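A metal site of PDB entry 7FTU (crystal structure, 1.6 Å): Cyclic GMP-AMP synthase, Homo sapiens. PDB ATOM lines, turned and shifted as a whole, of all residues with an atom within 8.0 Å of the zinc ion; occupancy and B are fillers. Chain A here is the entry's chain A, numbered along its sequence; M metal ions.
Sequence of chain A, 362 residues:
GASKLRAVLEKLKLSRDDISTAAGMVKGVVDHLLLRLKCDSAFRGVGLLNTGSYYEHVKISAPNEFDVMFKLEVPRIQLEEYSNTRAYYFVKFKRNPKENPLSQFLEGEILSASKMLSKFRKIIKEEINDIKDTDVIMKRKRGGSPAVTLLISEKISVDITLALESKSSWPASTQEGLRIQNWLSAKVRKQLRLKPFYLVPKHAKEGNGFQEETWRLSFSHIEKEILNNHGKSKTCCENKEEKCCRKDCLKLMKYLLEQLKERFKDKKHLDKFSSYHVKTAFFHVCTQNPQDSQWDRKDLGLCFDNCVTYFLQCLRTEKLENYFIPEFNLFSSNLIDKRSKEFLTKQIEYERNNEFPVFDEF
Four residues have an atom within 4 Å of the zinc ion: His 230, Cys 236, Cys 237 and Cys 244. The nearest printed residue that does not touch the zinc ion is Glu 242 (4.2 Å).
The side-chain amino group (NZ) of Lys 243 sits at hydrogen-bond distance from the backbone carbonyl oxygen (O) of Cys 237 (3.2 Å). NH2 of Arg 246 lies close to SG of Cys 244 (3.5 Å). The backbone carbonyl oxygen of Glu 242 is in hydrogen-bond range of the backbone NH of Cys 237, at 2.7 Å. O of Leu 227 sits at hydrogen-bond distance from ND1 of His 230 (3.0 Å). SG of Cys 236 lies close to NH2 of Arg 246 (3.7 Å).
The zinc ion is bound by NE2 of His 230 (2.1 Å), SG of Cys 237 (2.2 Å), SG of Cys 236 (2.3 Å) and SG of Cys 244 (2.4 Å). The zinc ion has four donor atoms within binding distance.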
ATOM      1  N   LEU A 227     -16.358  -1.154  20.133  1.00  0.00           N
ATOM      2  CA  LEU A 227     -17.350  -1.242  21.197  1.00  0.00           C
ATOM      3  C   LEU A 227     -17.505  -2.661  21.729  1.00  0.00           C
ATOM      4  O   LEU A 227     -17.828  -2.825  22.908  1.00  0.00           O
ATOM      5  CB  LEU A 227     -18.693  -0.680  20.704  1.00  0.00           C
ATOM      6  CG  LEU A 227     -18.827   0.842  20.797  1.00  0.00           C
ATOM      7  CD1 LEU A 227     -19.985   1.350  19.960  1.00  0.00           C
ATOM      8  CD2 LEU A 227     -18.985   1.295  22.228  1.00  0.00           C
ATOM      9  N   ASN A 229     -15.093  -4.881  21.828  1.00  0.00           N
ATOM     10  CA  ASN A 229     -13.802  -5.321  22.335  1.00  0.00           C
ATOM     11  C   ASN A 229     -13.096  -4.060  22.847  1.00  0.00           C
ATOM     12  O   ASN A 229     -12.148  -3.577  22.230  1.00  0.00           O
ATOM     13  CB  ASN A 229     -13.023  -6.085  21.260  1.00  0.00           C
ATOM     14  CG  ASN A 229     -11.801  -6.792  21.789  1.00  0.00           C
ATOM     15  OD1 ASN A 229     -11.528  -6.785  22.989  1.00  0.00           O
ATOM     16  ND2 ASN A 229     -11.066  -7.429  20.903  1.00  0.00           N
ATOM     17  N   HIS A 230     -13.620  -3.530  23.956  1.00  0.00           N
ATOM     18  CA  HIS A 230     -13.491  -2.116  24.278  1.00  0.00           C
ATOM     19  C   HIS A 230     -12.593  -1.851  25.492  1.00  0.00           C
ATOM     20  O   HIS A 230     -12.435  -0.696  25.884  1.00  0.00           O
ATOM     21  CB  HIS A 230     -14.870  -1.530  24.600  1.00  0.00           C
ATOM     22  CG  HIS A 230     -15.517  -2.224  25.742  1.00  0.00           C
ATOM     23  ND1 HIS A 230     -16.681  -2.946  25.668  1.00  0.00           N
ATOM     24  CD2 HIS A 230     -15.088  -2.341  27.010  1.00  0.00           C
ATOM     25  CE1 HIS A 230     -16.965  -3.443  26.864  1.00  0.00           C
ATOM     26  NE2 HIS A 230     -16.008  -3.074  27.695  1.00  0.00           N
ATOM     27  N   GLY A 231     -12.032  -2.885  26.116  1.00  0.00           N
ATOM     28  CA  GLY A 231     -11.251  -2.671  27.328  1.00  0.00           C
ATOM     29  C   GLY A 231      -9.753  -2.633  27.041  1.00  0.00           C
ATOM     30  O   GLY A 231      -9.320  -3.087  25.995  1.00  0.00           O
ATOM     31  N   LYS A 232      -8.964  -2.076  27.965  1.00  0.00           N
ATOM     32  CA  LYS A 232      -7.536  -2.287  27.959  1.00  0.00           C
ATOM     33  C   LYS A 232      -7.255  -3.769  28.243  1.00  0.00           C
ATOM     34  O   LYS A 232      -6.429  -4.377  27.569  1.00  0.00           O
ATOM     35  CB  LYS A 232      -6.823  -1.395  28.963  1.00  0.00           C
ATOM     36  CG  LYS A 232      -5.326  -1.677  29.084  1.00  0.00           C
ATOM     37  CD  LYS A 232      -4.557  -0.635  29.839  1.00  0.00           C
ATOM     38  CE  LYS A 232      -4.460   0.712  29.146  1.00  0.00           C
ATOM     39  NZ  LYS A 232      -3.880   0.594  27.785  1.00  0.00           N
ATOM     40  N   SER A 233      -7.952  -4.322  29.236  1.00  0.00           N
ATOM     41  CA  SER A 233      -7.890  -5.753  29.524  1.00  0.00           C
ATOM     42  C   SER A 233      -8.653  -6.495  28.440  1.00  0.00           C
ATOM     43  O   SER A 233      -9.765  -6.127  28.110  1.00  0.00           O
ATOM     44  CB  SER A 233      -8.451  -6.082  30.885  1.00  0.00           C
ATOM     45  OG  SER A 233      -8.672  -7.484  31.012  1.00  0.00           O
ATOM     46  N   THR A 235      -9.968  -9.231  28.828  1.00  0.00           N
ATOM     47  CA  THR A 235     -11.106  -9.894  29.468  1.00  0.00           C
ATOM     48  C   THR A 235     -12.126  -8.897  30.025  1.00  0.00           C
ATOM     49  O   THR A 235     -13.038  -9.284  30.745  1.00  0.00           O
ATOM     50  CB  THR A 235     -10.615 -10.939  30.481  1.00  0.00           C
ATOM     51  OG1 THR A 235      -9.743 -10.338  31.445  1.00  0.00           O
ATOM     52  CG2 THR A 235      -9.892 -12.086  29.807  1.00  0.00           C
ATOM     53  N   CYS A 236     -12.024  -7.612  29.643  1.00  0.00           N
ATOM     54  CA  CYS A 236     -13.005  -6.613  30.068  1.00  0.00           C
ATOM     55  C   CYS A 236     -14.414  -7.104  29.708  1.00  0.00           C
ATOM     56  O   CYS A 236     -14.663  -7.498  28.574  1.00  0.00           O
ATOM     57  CB  CYS A 236     -12.726  -5.252  29.442  1.00  0.00           C
ATOM     58  SG  CYS A 236     -13.562  -3.870  30.273  1.00  0.00           S
ATOM     59  N   CYS A 237     -15.288  -7.123  30.726  1.00  0.00           N
ATOM     60  CA  CYS A 237     -16.695  -7.509  30.640  1.00  0.00           C
ATOM     61  C   CYS A 237     -16.897  -8.997  30.317  1.00  0.00           C
ATOM     62  O   CYS A 237     -18.012  -9.410  30.002  1.00  0.00           O
ATOM     63  CB  CYS A 237     -17.451  -6.586  29.674  1.00  0.00           C
ATOM     64  SG  CYS A 237     -17.535  -4.879  30.274  1.00  0.00           S
ATOM     65  N   GLU A 238     -15.872  -9.845  30.472  1.00  0.00           N
ATOM     66  CA  GLU A 238     -16.037 -11.274  30.233  1.00  0.00           C
ATOM     67  C   GLU A 238     -16.283 -12.027  31.550  1.00  0.00           C
ATOM     68  O   GLU A 238     -16.604 -13.214  31.523  1.00  0.00           O
ATOM     69  CB  GLU A 238     -14.823 -11.897  29.554  1.00  0.00           C
ATOM     70  CG  GLU A 238     -14.773 -11.638  28.069  1.00  0.00           C
ATOM     71  CD  GLU A 238     -13.923 -12.616  27.287  1.00  0.00           C
ATOM     72  OE1 GLU A 238     -13.146 -13.372  27.929  1.00  0.00           O
ATOM     73  OE2 GLU A 238     -14.066 -12.644  26.055  1.00  0.00           O
ATOM     74  N   ASN A 239     -16.105 -11.350  32.685  1.00  0.00           N
ATOM     75  CA  ASN A 239     -16.350 -11.962  33.982  1.00  0.00           C
ATOM     76  C   ASN A 239     -16.906 -10.903  34.933  1.00  0.00           C
ATOM     77  O   ASN A 239     -16.787  -9.712  34.660  1.00  0.00           O
ATOM     78  CB  ASN A 239     -15.072 -12.606  34.517  1.00  0.00           C
ATOM     79  CG  ASN A 239     -13.961 -11.593  34.651  1.00  0.00           C
ATOM     80  OD1 ASN A 239     -13.993 -10.752  35.545  1.00  0.00           O
ATOM     81  ND2 ASN A 239     -12.987 -11.651  33.757  1.00  0.00           N
ATOM     82  N   GLU A 242     -14.749  -7.870  36.071  1.00  0.00           N
ATOM     83  CA  GLU A 242     -14.299  -6.836  35.140  1.00  0.00           C
ATOM     84  C   GLU A 242     -15.469  -6.230  34.361  1.00  0.00           C
ATOM     85  O   GLU A 242     -15.331  -5.961  33.176  1.00  0.00           O
ATOM     86  CB  GLU A 242     -13.279  -7.376  34.138  1.00  0.00           C
ATOM     87  CG  GLU A 242     -11.968  -7.862  34.739  1.00  0.00           C
ATOM     88  CD  GLU A 242     -10.978  -8.365  33.698  1.00  0.00           C
ATOM     89  OE1 GLU A 242     -10.415  -7.525  32.955  1.00  0.00           O
ATOM     90  OE2 GLU A 242     -10.802  -9.606  33.613  1.00  0.00           O
ATOM     91  N   LYS A 243     -16.585  -5.950  35.031  1.00  0.00           N
ATOM     92  CA  LYS A 243     -17.726  -5.302  34.393  1.00  0.00           C
ATOM     93  C   LYS A 243     -17.568  -3.778  34.407  1.00  0.00           C
ATOM     94  O   LYS A 243     -17.952  -3.136  35.382  1.00  0.00           O
ATOM     95  CB  LYS A 243     -19.009  -5.709  35.135  1.00  0.00           C
ATOM     96  CG  LYS A 243     -19.361  -7.181  35.037  1.00  0.00           C
ATOM     97  CD  LYS A 243     -19.723  -7.605  33.622  1.00  0.00           C
ATOM     98  CE  LYS A 243     -19.917  -9.097  33.478  1.00  0.00           C
ATOM     99  NZ  LYS A 243     -20.441  -9.433  32.132  1.00  0.00           N
ATOM    100  N   CYS A 244     -17.020  -3.184  33.338  1.00  0.00           N
ATOM    101  CA  CYS A 244     -16.832  -1.736  33.286  1.00  0.00           C
ATOM    102  C   CYS A 244     -18.160  -1.062  32.968  1.00  0.00           C
ATOM    103  O   CYS A 244     -19.144  -1.738  32.649  1.00  0.00           O
ATOM    104  CB  CYS A 244     -15.741  -1.355  32.282  1.00  0.00           C
ATOM    105  SG  CYS A 244     -16.246  -1.417  30.541  1.00  0.00           S
ATOM    106  N   CYS A 245     -18.194   0.271  33.040  1.00  0.00           N
ATOM    107  CA  CYS A 245     -19.425   1.013  32.806  1.00  0.00           C
ATOM    108  C   CYS A 245     -19.355   1.817  31.507  1.00  0.00           C
ATOM    109  O   CYS A 245     -20.179   2.713  31.303  1.00  0.00           O
ATOM    110  CB  CYS A 245     -19.761   1.911  34.006  1.00  0.00           C
ATOM    111  SG  CYS A 245     -18.591   3.255  34.288  1.00  0.00           S
ATOM    112  N   ARG A 246     -18.454   1.457  30.584  1.00  0.00           N
ATOM    113  CA  ARG A 246     -18.317   2.152  29.308  1.00  0.00           C
ATOM    114  C   ARG A 246     -19.632   2.138  28.526  1.00  0.00           C
ATOM    115  O   ARG A 246     -20.110   3.202  28.124  1.00  0.00           O
ATOM    116  CB  ARG A 246     -17.180   1.549  28.476  1.00  0.00           C
ATOM    117  CG  ARG A 246     -15.790   1.966  28.923  1.00  0.00           C
ATOM    118  CD  ARG A 246     -14.746   1.507  27.936  1.00  0.00           C
ATOM    119  NE  ARG A 246     -13.368   1.727  28.357  1.00  0.00           N
ATOM    120  CZ  ARG A 246     -12.630   0.856  29.059  1.00  0.00           C
ATOM    121  NH1 ARG A 246     -11.355   1.126  29.258  1.00  0.00           N
ATOM    122  NH2 ARG A 246     -13.142  -0.266  29.541  1.00  0.00           N
ATOM    123  N   LYS A 247     -20.217   0.955  28.312  1.00  0.00           N
ATOM    124  CA  LYS A 247     -21.419   0.875  27.492  1.00  0.00           C
ATOM    125  C   LYS A 247     -22.602   1.543  28.206  1.00  0.00           C
ATOM    126  O   LYS A 247     -23.446   2.174  27.567  1.00  0.00           O
ATOM    127  CB  LYS A 247     -21.727  -0.554  27.062  1.00  0.00           C
ATOM    128  CG  LYS A 247     -20.749  -1.107  26.037  1.00  0.00           C
ATOM    129  CD  LYS A 247     -21.296  -2.284  25.239  1.00  0.00           C
ATOM    130  CE  LYS A 247     -20.330  -2.717  24.161  1.00  0.00           C
ATOM    131  NZ  LYS A 247     -20.765  -3.936  23.455  1.00  0.00           N
ATOM    132  N   ASP A 292      -9.185   0.569  32.380  1.00  0.00           N
ATOM    133  CA  ASP A 292     -10.479   0.035  32.772  1.00  0.00           C
ATOM    134  C   ASP A 292     -10.859   0.519  34.171  1.00  0.00           C
ATOM    135  O   ASP A 292     -12.052   0.608  34.486  1.00  0.00           O
ATOM    136  CB  ASP A 292     -10.484  -1.492  32.698  1.00  0.00           C
ATOM    137  CG  ASP A 292     -10.219  -2.035  31.300  1.00  0.00           C
ATOM    138  OD1 ASP A 292     -10.427  -1.291  30.327  1.00  0.00           O
ATOM    139  OD2 ASP A 292      -9.741  -3.181  31.202  1.00  0.00           O
ATOM    140  N   TRP A 295     -13.315   3.266  34.544  1.00  0.00           N
ATOM    141  CA  TRP A 295     -14.668   2.914  34.126  1.00  0.00           C
ATOM    142  C   TRP A 295     -15.226   1.853  35.058  1.00  0.00           C
ATOM    143  O   TRP A 295     -15.937   0.950  34.633  1.00  0.00           O
ATOM    144  CB  TRP A 295     -14.687   2.458  32.666  1.00  0.00           C
ATOM    145  CG  TRP A 295     -14.222   3.498  31.710  1.00  0.00           C
ATOM    146  CD1 TRP A 295     -12.953   3.681  31.234  1.00  0.00           C
ATOM    147  CD2 TRP A 295     -15.021   4.525  31.119  1.00  0.00           C
ATOM    148  NE1 TRP A 295     -12.911   4.748  30.387  1.00  0.00           N
ATOM    149  CE2 TRP A 295     -14.168   5.294  30.296  1.00  0.00           C
ATOM    150  CE3 TRP A 295     -16.371   4.873  31.202  1.00  0.00           C
ATOM    151  CZ2 TRP A 295     -14.634   6.366  29.524  1.00  0.00           C
ATOM    152  CZ3 TRP A 295     -16.832   5.944  30.461  1.00  0.00           C
ATOM    153  CH2 TRP A 295     -15.976   6.681  29.636  1.00  0.00           C
HETATM  154 ZN    ZN M   1     -15.816  -3.578  29.691  1.00  0.00          ZN
